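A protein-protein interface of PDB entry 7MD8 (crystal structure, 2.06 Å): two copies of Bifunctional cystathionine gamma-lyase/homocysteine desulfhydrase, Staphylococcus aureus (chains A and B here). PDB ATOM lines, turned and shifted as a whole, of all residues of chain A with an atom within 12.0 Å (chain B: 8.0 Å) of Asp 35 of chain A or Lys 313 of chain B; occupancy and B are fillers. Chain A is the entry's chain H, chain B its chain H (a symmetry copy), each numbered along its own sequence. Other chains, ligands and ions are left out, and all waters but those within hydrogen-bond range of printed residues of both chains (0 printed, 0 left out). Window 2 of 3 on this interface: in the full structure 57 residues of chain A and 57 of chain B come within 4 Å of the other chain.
Of the printed residues of chain B, Asp 35 of chain A touches Lys 313 and Leu 320.
Lys 313 of chain B touches just these residues of chain A: Asp 34 (3.2 Å) and Asp 35 (3.1 Å).
No residue of chain A comes within 4 Å of Gln 310 of chain B.
No residue of chain A comes within 4 Å of Ala 314 of chain B.
No residue of chain A comes within 4 Å of Thr 315 of chain B.
No residue of chain A comes within 4 Å of Ser 316 of chain B.
Of the printed residues of chain B, Ile 36 of chain A touches Ile 312, Leu 320 and Met 337.
Printed residues of chain A within 4 Å of Met 337 of chain B: Ile 36.
Ala 376 of chain B touches none of the printed residues of chain A.
Thr 30 of chain A touches none of the printed residues of chain B.
The nearest residue of chain B that does not touch Asp 35 of chain A is Lys 309 of chain B (6.8 Å).
The side-chain amide oxygen (OE1) of Gln 33 of chain A sits at hydrogen-bond distance from the backbone NH (N) of Gly 37 of chain A (3.1 Å).
OD1 of Asp 34 of chain A is in salt-bridge range of NH2 of Arg 40 of chain A, at 3.1 Å.
The backbone carbonyl oxygen of Ile 312 of chain B is in hydrogen-bond range of the side-chain hydroxyl of Thr 315 of chain B (3.0 Å).
Hydrophobic or aromatic side chains of chain A that line the printed part of chain B: Ile 36.
Along chain A the printed residues that touch a printed residue of chain B span positions 32 to 36.
Of the 19 printed residues of chain B, 4 touch a printed residue of chain A.
Hydrophobic or aromatic side chains of chain B within 4 Å of the printed part of chain A: Ile 312, Leu 320 and Met 337.
Among the printed residues, 8 pairs touch across the chains.
Among the printed residues, Asp or Glu carboxylates within 4 Å of a Lys or Arg side-chain nitrogen of the other chain: Asp 35 of chain A with Lys 313 of chain B.
Among the printed residues, pairs that only touch across the chains: Leu 32 of chain A with Leu 320 of chain B (3.8 Å), Asp 35 of chain A with Leu 320 of chain B (3.8 Å), Ile 36 of chain A with Ile 312 of chain B (3.8 Å), Ile 36 of chain A with Leu 320 of chain B (3.6 Å) and Ile 36 of chain A with Met 337 of chain B (3.6 Å).
The backbone carbonyl oxygen of Leu 320 of chain B is in hydrogen-bond range of the backbone NH of Gln 33 of chain A, at 3.0 Å.
The side-chain amino group (NZ) of Lys 313 of chain B sits at hydrogen-bond distance from the backbone carbonyl oxygen (O) of Asp 34 of chain A (3.2 Å).
The side-chain amino group (NZ) of Lys 313 of chain B is in salt-bridge range of the side-chain carboxylate (OD1) of Asp 35 of chain A.
No position is printed for both chains.
Of the 8 pairs that touch across the chains among the printed residues, none has its exchanged pair printed and touching as well.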
ATOM      1  N   THR A  30      -4.624   0.233  12.694  1.00  0.00           N
ATOM      2  CA  THR A  30      -3.407   1.007  12.906  1.00  0.00           C
ATOM      3  C   THR A  30      -3.595   2.417  12.354  1.00  0.00           C
ATOM      4  O   THR A  30      -4.576   2.714  11.659  1.00  0.00           O
ATOM      5  CB  THR A  30      -2.194   0.298  12.284  1.00  0.00           C
ATOM      6  OG1 THR A  30      -0.999   0.987  12.651  1.00  0.00           O
ATOM      7  CG2 THR A  30      -2.297   0.266  10.784  1.00  0.00           C
ATOM      8  N   TYR A  31      -2.651   3.301  12.704  1.00  0.00           N
ATOM      9  CA  TYR A  31      -2.818   4.743  12.540  1.00  0.00           C
ATOM     10  C   TYR A  31      -1.534   5.371  12.016  1.00  0.00           C
ATOM     11  O   TYR A  31      -0.431   5.023  12.460  1.00  0.00           O
ATOM     12  CB  TYR A  31      -3.230   5.415  13.869  1.00  0.00           C
ATOM     13  CG  TYR A  31      -4.466   4.781  14.470  1.00  0.00           C
ATOM     14  CD1 TYR A  31      -4.375   3.586  15.186  1.00  0.00           C
ATOM     15  CD2 TYR A  31      -5.730   5.349  14.285  1.00  0.00           C
ATOM     16  CE1 TYR A  31      -5.499   2.977  15.704  1.00  0.00           C
ATOM     17  CE2 TYR A  31      -6.867   4.741  14.807  1.00  0.00           C
ATOM     18  CZ  TYR A  31      -6.735   3.544  15.512  1.00  0.00           C
ATOM     19  OH  TYR A  31      -7.836   2.914  16.043  1.00  0.00           O
ATOM     20  N   LEU A  32      -1.696   6.288  11.056  1.00  0.00           N
ATOM     21  CA  LEU A  32      -0.576   7.058  10.522  1.00  0.00           C
ATOM     22  C   LEU A  32       0.113   7.832  11.634  1.00  0.00           C
ATOM     23  O   LEU A  32      -0.543   8.427  12.494  1.00  0.00           O
ATOM     24  CB  LEU A  32      -1.061   8.055   9.457  1.00  0.00           C
ATOM     25  CG  LEU A  32      -1.801   7.529   8.230  1.00  0.00           C
ATOM     26  CD1 LEU A  32      -2.447   8.640   7.388  1.00  0.00           C
ATOM     27  CD2 LEU A  32      -0.848   6.768   7.397  1.00  0.00           C
ATOM     28  N   GLN A  33       1.441   7.852  11.601  1.00  0.00           N
ATOM     29  CA  GLN A  33       2.220   8.727  12.471  1.00  0.00           C
ATOM     30  C   GLN A  33       2.905   9.798  11.625  1.00  0.00           C
ATOM     31  O   GLN A  33       3.567   9.480  10.631  1.00  0.00           O
ATOM     32  CB  GLN A  33       3.244   7.926  13.277  1.00  0.00           C
ATOM     33  CG  GLN A  33       2.604   6.920  14.235  1.00  0.00           C
ATOM     34  CD  GLN A  33       3.628   6.166  15.061  1.00  0.00           C
ATOM     35  OE1 GLN A  33       4.729   6.659  15.303  1.00  0.00           O
ATOM     36  NE2 GLN A  33       3.270   4.965  15.499  1.00  0.00           N
ATOM     37  N   ASP A  34       2.721  11.066  12.006  1.00  0.00           N
ATOM     38  CA  ASP A  34       3.351  12.154  11.257  1.00  0.00           C
ATOM     39  C   ASP A  34       4.860  12.178  11.479  1.00  0.00           C
ATOM     40  O   ASP A  34       5.625  12.478  10.557  1.00  0.00           O
ATOM     41  CB  ASP A  34       2.721  13.491  11.643  1.00  0.00           C
ATOM     42  CG  ASP A  34       1.267  13.588  11.211  1.00  0.00           C
ATOM     43  OD1 ASP A  34       0.951  13.116  10.097  1.00  0.00           O
ATOM     44  OD2 ASP A  34       0.443  14.115  11.989  1.00  0.00           O
ATOM     45  N   ASP A  35       5.303  11.865  12.692  1.00  0.00           N
ATOM     46  CA  ASP A  35       6.705  11.614  12.988  1.00  0.00           C
ATOM     47  C   ASP A  35       6.757  10.458  13.965  1.00  0.00           C
ATOM     48  O   ASP A  35       5.803  10.232  14.713  1.00  0.00           O
ATOM     49  CB  ASP A  35       7.410  12.848  13.575  1.00  0.00           C
ATOM     50  CG  ASP A  35       7.444  14.017  12.601  1.00  0.00           C
ATOM     51  OD1 ASP A  35       8.282  13.985  11.671  1.00  0.00           O
ATOM     52  OD2 ASP A  35       6.622  14.956  12.750  1.00  0.00           O
ATOM     53  N   ILE A  36       7.865   9.719  13.946  1.00  0.00           N
ATOM     54  CA  ILE A  36       8.029   8.588  14.855  1.00  0.00           C
ATOM     55  C   ILE A  36       7.702   9.028  16.276  1.00  0.00           C
ATOM     56  O   ILE A  36       8.342   9.936  16.816  1.00  0.00           O
ATOM     57  CB  ILE A  36       9.445   7.999  14.779  1.00  0.00           C
ATOM     58  CG1 ILE A  36       9.716   7.448  13.386  1.00  0.00           C
ATOM     59  CG2 ILE A  36       9.612   6.911  15.830  1.00  0.00           C
ATOM     60  CD1 ILE A  36      11.063   6.778  13.251  1.00  0.00           C
ATOM     61  N   GLY A  37       6.682   8.405  16.875  1.00  0.00           N
ATOM     62  CA  GLY A  37       6.254   8.724  18.222  1.00  0.00           C
ATOM     63  C   GLY A  37       5.221   9.826  18.323  1.00  0.00           C
ATOM     64  O   GLY A  37       4.678  10.051  19.414  1.00  0.00           O
ATOM     65  N   ASP A  38       4.936  10.525  17.229  1.00  0.00           N
ATOM     66  CA  ASP A  38       3.953  11.598  17.211  1.00  0.00           C
ATOM     67  C   ASP A  38       2.629  10.988  16.762  1.00  0.00           C
ATOM     68  O   ASP A  38       2.470  10.620  15.593  1.00  0.00           O
ATOM     69  CB  ASP A  38       4.412  12.723  16.279  1.00  0.00           C
ATOM     70  CG  ASP A  38       3.481  13.950  16.287  1.00  0.00           C
ATOM     71  OD1 ASP A  38       2.355  13.903  16.853  1.00  0.00           O
ATOM     72  OD2 ASP A  38       3.885  14.979  15.693  1.00  0.00           O
ATOM     73  N   LEU A  39       1.690  10.872  17.692  1.00  0.00           N
ATOM     74  CA  LEU A  39       0.350  10.393  17.401  1.00  0.00           C
ATOM     75  C   LEU A  39      -0.594  11.587  17.278  1.00  0.00           C
ATOM     76  O   LEU A  39      -0.631  12.448  18.165  1.00  0.00           O
ATOM     77  CB  LEU A  39      -0.123   9.434  18.499  1.00  0.00           C
ATOM     78  CG  LEU A  39       0.866   8.351  18.959  1.00  0.00           C
ATOM     79  CD1 LEU A  39       0.248   7.464  20.026  1.00  0.00           C
ATOM     80  CD2 LEU A  39       1.334   7.509  17.790  1.00  0.00           C
ATOM     81  N   ARG A  40      -1.357  11.628  16.181  1.00  0.00           N
ATOM     82  CA  ARG A  40      -2.252  12.754  15.909  1.00  0.00           C
ATOM     83  C   ARG A  40      -3.256  12.967  17.028  1.00  0.00           C
ATOM     84  O   ARG A  40      -3.458  14.096  17.488  1.00  0.00           O
ATOM     85  CB  ARG A  40      -3.009  12.517  14.606  1.00  0.00           C
ATOM     86  CG  ARG A  40      -2.149  12.473  13.397  1.00  0.00           C
ATOM     87  CD  ARG A  40      -2.989  12.558  12.142  1.00  0.00           C
ATOM     88  NE  ARG A  40      -2.107  12.420  10.995  1.00  0.00           N
ATOM     89  CZ  ARG A  40      -2.509  12.157   9.763  1.00  0.00           C
ATOM     90  NH1 ARG A  40      -3.804  11.987   9.502  1.00  0.00           N
ATOM     91  NH2 ARG A  40      -1.607  12.056   8.798  1.00  0.00           N
ATOM     92  N   GLN A  41      -3.956  11.904  17.429  1.00  0.00           N
ATOM     93  CA  GLN A  41      -4.971  12.003  18.473  1.00  0.00           C
ATOM     94  C   GLN A  41      -4.761  10.959  19.553  1.00  0.00           C
ATOM     95  O   GLN A  41      -5.717  10.606  20.257  1.00  0.00           O
ATOM     96  CB  GLN A  41      -6.380  11.872  17.890  1.00  0.00           C
ATOM     97  CG  GLN A  41      -6.729  12.994  16.966  1.00  0.00           C
ATOM     98  CD  GLN A  41      -6.938  14.302  17.702  1.00  0.00           C
ATOM     99  OE1 GLN A  41      -7.397  14.320  18.843  1.00  0.00           O
ATOM    100  NE2 GLN A  41      -6.601  15.407  17.046  1.00  0.00           N
ATOM    101  N   GLY A  42      -3.536  10.452  19.686  1.00  0.00           N
ATOM    102  CA  GLY A  42      -3.213   9.493  20.713  1.00  0.00           C
ATOM    103  C   GLY A  42      -3.437   8.050  20.336  1.00  0.00           C
ATOM    104  O   GLY A  42      -3.281   7.174  21.192  1.00  0.00           O
ATOM    105  N   TYR A  43      -3.805   7.769  19.090  1.00  0.00           N
ATOM    106  CA  TYR A  43      -4.035   6.404  18.650  1.00  0.00           C
ATOM    107  C   TYR A  43      -2.831   5.913  17.867  1.00  0.00           C
ATOM    108  O   TYR A  43      -2.236   6.664  17.086  1.00  0.00           O
ATOM    109  CB  TYR A  43      -5.311   6.308  17.814  1.00  0.00           C
ATOM    110  CG  TYR A  43      -6.521   6.633  18.658  1.00  0.00           C
ATOM    111  CD1 TYR A  43      -7.102   5.659  19.457  1.00  0.00           C
ATOM    112  CD2 TYR A  43      -7.055   7.921  18.696  1.00  0.00           C
ATOM    113  CE1 TYR A  43      -8.190   5.941  20.257  1.00  0.00           C
ATOM    114  CE2 TYR A  43      -8.154   8.215  19.491  1.00  0.00           C
ATOM    115  CZ  TYR A  43      -8.709   7.210  20.273  1.00  0.00           C
ATOM    116  OH  TYR A  43      -9.785   7.447  21.079  1.00  0.00           O
ATOM    117  N   GLU A  44      -2.457   4.659  18.104  1.00  0.00           N
ATOM    118  CA  GLU A  44      -1.352   4.059  17.373  1.00  0.00           C
ATOM    119  C   GLU A  44      -1.587   2.614  16.976  1.00  0.00           C
ATOM    120  O   GLU A  44      -0.989   2.173  15.986  1.00  0.00           O
ATOM    121  CB  GLU A  44      -0.058   4.155  18.188  1.00  0.00           C
ATOM    122  CG  GLU A  44       0.126   3.065  19.184  1.00  0.00           C
ATOM    123  CD  GLU A  44       1.227   3.375  20.190  1.00  0.00           C
ATOM    124  OE1 GLU A  44       0.894   3.556  21.384  1.00  0.00           O
ATOM    125  OE2 GLU A  44       2.408   3.446  19.778  1.00  0.00           O
ATOM    126  N   GLU B 306      19.298   9.420  12.083  1.00  0.00           N
ATOM    127  CA  GLU B 306      18.899  10.491  11.179  1.00  0.00           C
ATOM    128  C   GLU B 306      18.762   9.970   9.753  1.00  0.00           C
ATOM    129  O   GLU B 306      17.861  10.392   9.019  1.00  0.00           O
ATOM    130  CB  GLU B 306      19.898  11.645  11.260  1.00  0.00           C
ATOM    131  CG  GLU B 306      19.423  12.930  10.589  1.00  0.00           C
ATOM    132  N   SER B 307      19.618   9.017   9.363  1.00  0.00           N
ATOM    133  CA  SER B 307      19.471   8.363   8.063  1.00  0.00           C
ATOM    134  C   SER B 307      18.139   7.629   7.959  1.00  0.00           C
ATOM    135  O   SER B 307      17.465   7.693   6.924  1.00  0.00           O
ATOM    136  CB  SER B 307      20.616   7.384   7.838  1.00  0.00           C
ATOM    137  OG  SER B 307      21.810   8.067   7.518  1.00  0.00           O
ATOM    138  N   ALA B 308      17.743   6.931   9.030  1.00  0.00           N
ATOM    139  CA  ALA B 308      16.488   6.185   9.023  1.00  0.00           C
ATOM    140  C   ALA B 308      15.297   7.124   8.894  1.00  0.00           C
ATOM    141  O   ALA B 308      14.368   6.879   8.102  1.00  0.00           O
ATOM    142  CB  ALA B 308      16.380   5.338  10.296  1.00  0.00           C
ATOM    143  N   LYS B 309      15.313   8.219   9.662  1.00  0.00           N
ATOM    144  CA  LYS B 309      14.238   9.202   9.577  1.00  0.00           C
ATOM    145  C   LYS B 309      14.182   9.844   8.193  1.00  0.00           C
ATOM    146  O   LYS B 309      13.093  10.048   7.640  1.00  0.00           O
ATOM    147  CB  LYS B 309      14.414  10.263  10.658  1.00  0.00           C
ATOM    148  CG  LYS B 309      14.087   9.766  12.056  1.00  0.00           C
ATOM    149  CD  LYS B 309      14.190  10.889  13.075  1.00  0.00           C
ATOM    150  CE  LYS B 309      13.681  10.441  14.438  1.00  0.00           C
ATOM    151  NZ  LYS B 309      13.902  11.480  15.476  1.00  0.00           N
ATOM    152  N   GLN B 310      15.345  10.160   7.616  1.00  0.00           N
ATOM    153  CA  GLN B 310      15.390  10.745   6.280  1.00  0.00           C
ATOM    154  C   GLN B 310      14.798   9.792   5.250  1.00  0.00           C
ATOM    155  O   GLN B 310      14.006  10.203   4.391  1.00  0.00           O
ATOM    156  CB  GLN B 310      16.840  11.115   5.940  1.00  0.00           C
ATOM    157  CG  GLN B 310      17.131  11.492   4.481  1.00  0.00           C
ATOM    158  CD  GLN B 310      16.256  12.625   3.944  1.00  0.00           C
ATOM    159  OE1 GLN B 310      15.830  13.517   4.689  1.00  0.00           O
ATOM    160  NE2 GLN B 310      15.989  12.592   2.634  1.00  0.00           N
ATOM    161  N   LEU B 311      15.163   8.510   5.331  1.00  0.00           N
ATOM    162  CA  LEU B 311      14.549   7.486   4.491  1.00  0.00           C
ATOM    163  C   LEU B 311      13.027   7.543   4.577  1.00  0.00           C
ATOM    164  O   LEU B 311      12.329   7.581   3.556  1.00  0.00           O
ATOM    165  CB  LEU B 311      15.058   6.111   4.922  1.00  0.00           C
ATOM    166  CG  LEU B 311      14.820   4.948   3.973  1.00  0.00           C
ATOM    167  CD1 LEU B 311      15.423   5.300   2.637  1.00  0.00           C
ATOM    168  CD2 LEU B 311      15.474   3.687   4.534  1.00  0.00           C
ATOM    169  N   ILE B 312      12.494   7.549   5.802  1.00  0.00           N
ATOM    170  CA  ILE B 312      11.042   7.583   5.966  1.00  0.00           C
ATOM    171  C   ILE B 312      10.455   8.831   5.316  1.00  0.00           C
ATOM    172  O   ILE B 312       9.427   8.766   4.628  1.00  0.00           O
ATOM    173  CB  ILE B 312      10.670   7.500   7.456  1.00  0.00           C
ATOM    174  CG1 ILE B 312      10.929   6.093   7.995  1.00  0.00           C
ATOM    175  CG2 ILE B 312       9.217   7.914   7.670  1.00  0.00           C
ATOM    176  CD1 ILE B 312      10.771   5.990   9.510  1.00  0.00           C
ATOM    177  N   LYS B 313      11.096   9.987   5.524  1.00  0.00           N
ATOM    178  CA  LYS B 313      10.578  11.244   4.986  1.00  0.00           C
ATOM    179  C   LYS B 313      10.608  11.273   3.460  1.00  0.00           C
ATOM    180  O   LYS B 313       9.746  11.900   2.838  1.00  0.00           O
ATOM    181  CB  LYS B 313      11.376  12.425   5.545  1.00  0.00           C
ATOM    182  CG  LYS B 313      10.909  12.941   6.912  1.00  0.00           C
ATOM    183  CD  LYS B 313       9.387  13.143   6.982  1.00  0.00           C
ATOM    184  CE  LYS B 313       8.919  13.420   8.420  1.00  0.00           C
ATOM    185  NZ  LYS B 313       8.411  12.176   9.106  1.00  0.00           N
ATOM    186  N   ALA B 314      11.576  10.599   2.840  1.00  0.00           N
ATOM    187  CA  ALA B 314      11.787  10.721   1.405  1.00  0.00           C
ATOM    188  C   ALA B 314      10.993   9.724   0.570  1.00  0.00           C
ATOM    189  O   ALA B 314      10.930   9.887  -0.651  1.00  0.00           O
ATOM    190  CB  ALA B 314      13.277  10.565   1.081  1.00  0.00           C
ATOM    191  N   THR B 315      10.416   8.687   1.173  1.00  0.00           N
ATOM    192  CA  THR B 315       9.655   7.701   0.417  1.00  0.00           C
ATOM    193  C   THR B 315       8.243   8.208   0.155  1.00  0.00           C
ATOM    194  O   THR B 315       7.593   8.773   1.040  1.00  0.00           O
ATOM    195  CB  THR B 315       9.574   6.362   1.160  1.00  0.00           C
ATOM    196  OG1 THR B 315       9.199   6.590   2.524  1.00  0.00           O
ATOM    197  CG2 THR B 315      10.891   5.601   1.105  1.00  0.00           C
ATOM    198  N   SER B 316       7.760   7.983  -1.063  1.00  0.00           N
ATOM    199  CA  SER B 316       6.395   8.366  -1.381  1.00  0.00           C
ATOM    200  C   SER B 316       5.387   7.282  -1.017  1.00  0.00           C
ATOM    201  O   SER B 316       4.260   7.602  -0.629  1.00  0.00           O
ATOM    202  CB  SER B 316       6.291   8.702  -2.870  1.00  0.00           C
ATOM    203  OG  SER B 316       6.772  10.014  -3.102  1.00  0.00           O
ATOM    204  N   TYR B 318       5.908   4.374   1.146  1.00  0.00           N
ATOM    205  CA  TYR B 318       6.067   3.630   2.393  1.00  0.00           C
ATOM    206  C   TYR B 318       5.493   4.451   3.538  1.00  0.00           C
ATOM    207  O   TYR B 318       5.940   5.575   3.785  1.00  0.00           O
ATOM    208  CB  TYR B 318       7.532   3.295   2.658  1.00  0.00           C
ATOM    209  CG  TYR B 318       8.119   2.356   1.641  1.00  0.00           C
ATOM    210  CD1 TYR B 318       8.481   2.809   0.379  1.00  0.00           C
ATOM    211  CD2 TYR B 318       8.305   1.017   1.938  1.00  0.00           C
ATOM    212  CE1 TYR B 318       9.016   1.946  -0.559  1.00  0.00           C
ATOM    213  CE2 TYR B 318       8.843   0.149   1.012  1.00  0.00           C
ATOM    214  CZ  TYR B 318       9.198   0.620  -0.234  1.00  0.00           C
ATOM    215  OH  TYR B 318       9.732  -0.243  -1.162  1.00  0.00           O
ATOM    216  N   LEU B 320       4.482   5.355   7.441  1.00  0.00           N
ATOM    217  CA  LEU B 320       4.948   5.209   8.817  1.00  0.00           C
ATOM    218  C   LEU B 320       3.760   4.861   9.710  1.00  0.00           C
ATOM    219  O   LEU B 320       2.918   5.719  10.006  1.00  0.00           O
ATOM    220  CB  LEU B 320       5.630   6.484   9.298  1.00  0.00           C
ATOM    221  CG  LEU B 320       6.057   6.426  10.767  1.00  0.00           C
ATOM    222  CD1 LEU B 320       7.156   5.374  10.947  1.00  0.00           C
ATOM    223  CD2 LEU B 320       6.513   7.794  11.257  1.00  0.00           C
ATOM    224  N   ILE B 331       6.575   1.182   7.012  1.00  0.00           N
ATOM    225  CA  ILE B 331       7.968   1.385   7.365  1.00  0.00           C
ATOM    226  C   ILE B 331       8.024   1.784   8.831  1.00  0.00           C
ATOM    227  O   ILE B 331       7.111   2.439   9.346  1.00  0.00           O
ATOM    228  CB  ILE B 331       8.629   2.441   6.449  1.00  0.00           C
ATOM    229  CG1 ILE B 331      10.141   2.503   6.695  1.00  0.00           C
ATOM    230  CG2 ILE B 331       7.939   3.795   6.616  1.00  0.00           C
ATOM    231  CD1 ILE B 331      10.957   2.904   5.470  1.00  0.00           C
ATOM    232  N   MET B 337      10.722   2.303  18.044  1.00  0.00           N
ATOM    233  CA  MET B 337       9.288   2.052  18.088  1.00  0.00           C
ATOM    234  C   MET B 337       8.909   0.771  18.811  1.00  0.00           C
ATOM    235  O   MET B 337       7.803   0.691  19.343  1.00  0.00           O
ATOM    236  CB  MET B 337       8.705   2.029  16.658  1.00  0.00           C
ATOM    237  CG  MET B 337       8.768   3.387  15.939  1.00  0.00           C
ATOM    238  SD  MET B 337       8.315   3.358  14.179  1.00  0.00           S
ATOM    239  CE  MET B 337       6.610   2.813  14.273  1.00  0.00           C
ATOM    240  N   ASP B 372      10.964   3.848  -5.556  1.00  0.00           N
ATOM    241  CA  ASP B 372      10.733   4.779  -4.459  1.00  0.00           C
ATOM    242  C   ASP B 372      11.762   4.577  -3.350  1.00  0.00           C
ATOM    243  O   ASP B 372      12.388   5.542  -2.878  1.00  0.00           O
ATOM    244  CB  ASP B 372       9.316   4.588  -3.925  1.00  0.00           C
ATOM    245  CG  ASP B 372       8.909   5.657  -2.931  1.00  0.00           C
ATOM    246  OD1 ASP B 372       9.262   6.838  -3.130  1.00  0.00           O
ATOM    247  OD2 ASP B 372       8.192   5.323  -1.963  1.00  0.00           O
ATOM    248  N   GLN B 375      15.358   5.678  -4.623  1.00  0.00           N
ATOM    249  CA  GLN B 375      15.604   7.122  -4.682  1.00  0.00           C
ATOM    250  C   GLN B 375      15.685   7.720  -3.282  1.00  0.00           C
ATOM    251  O   GLN B 375      16.501   8.629  -3.027  1.00  0.00           O
ATOM    252  CB  GLN B 375      14.533   7.837  -5.529  1.00  0.00           C
ATOM    253  CG  GLN B 375      13.097   7.779  -4.988  1.00  0.00           C
ATOM    254  CD  GLN B 375      12.797   8.842  -3.913  1.00  0.00           C
ATOM    255  OE1 GLN B 375      13.470   9.875  -3.822  1.00  0.00           O
ATOM    256  NE2 GLN B 375      11.795   8.569  -3.081  1.00  0.00           N
ATOM    257  N   ALA B 376      14.870   7.204  -2.347  1.00  0.00           N
ATOM    258  CA  ALA B 376      14.979   7.672  -0.967  1.00  0.00           C
ATOM    259  C   ALA B 376      16.358   7.363  -0.390  1.00  0.00           C
ATOM    260  O   ALA B 376      16.983   8.227   0.235  1.00  0.00           O
ATOM    261  CB  ALA B 376      13.876   7.058  -0.111  1.00  0.00           C
ATOM    262  N   THR B 379      19.022   9.688  -1.491  1.00  0.00           N
ATOM    263  CA  THR B 379      19.165  10.962  -0.779  1.00  0.00           C
ATOM    264  C   THR B 379      20.064  10.884   0.452  1.00  0.00           C
ATOM    265  O   THR B 379      20.339  11.925   1.060  1.00  0.00           O
ATOM    266  CB  THR B 379      17.815  11.530  -0.336  1.00  0.00           C
ATOM    267  OG1 THR B 379      17.387  10.888   0.874  1.00  0.00           O
ATOM    268  CG2 THR B 379      16.764  11.397  -1.445  1.00  0.00           C
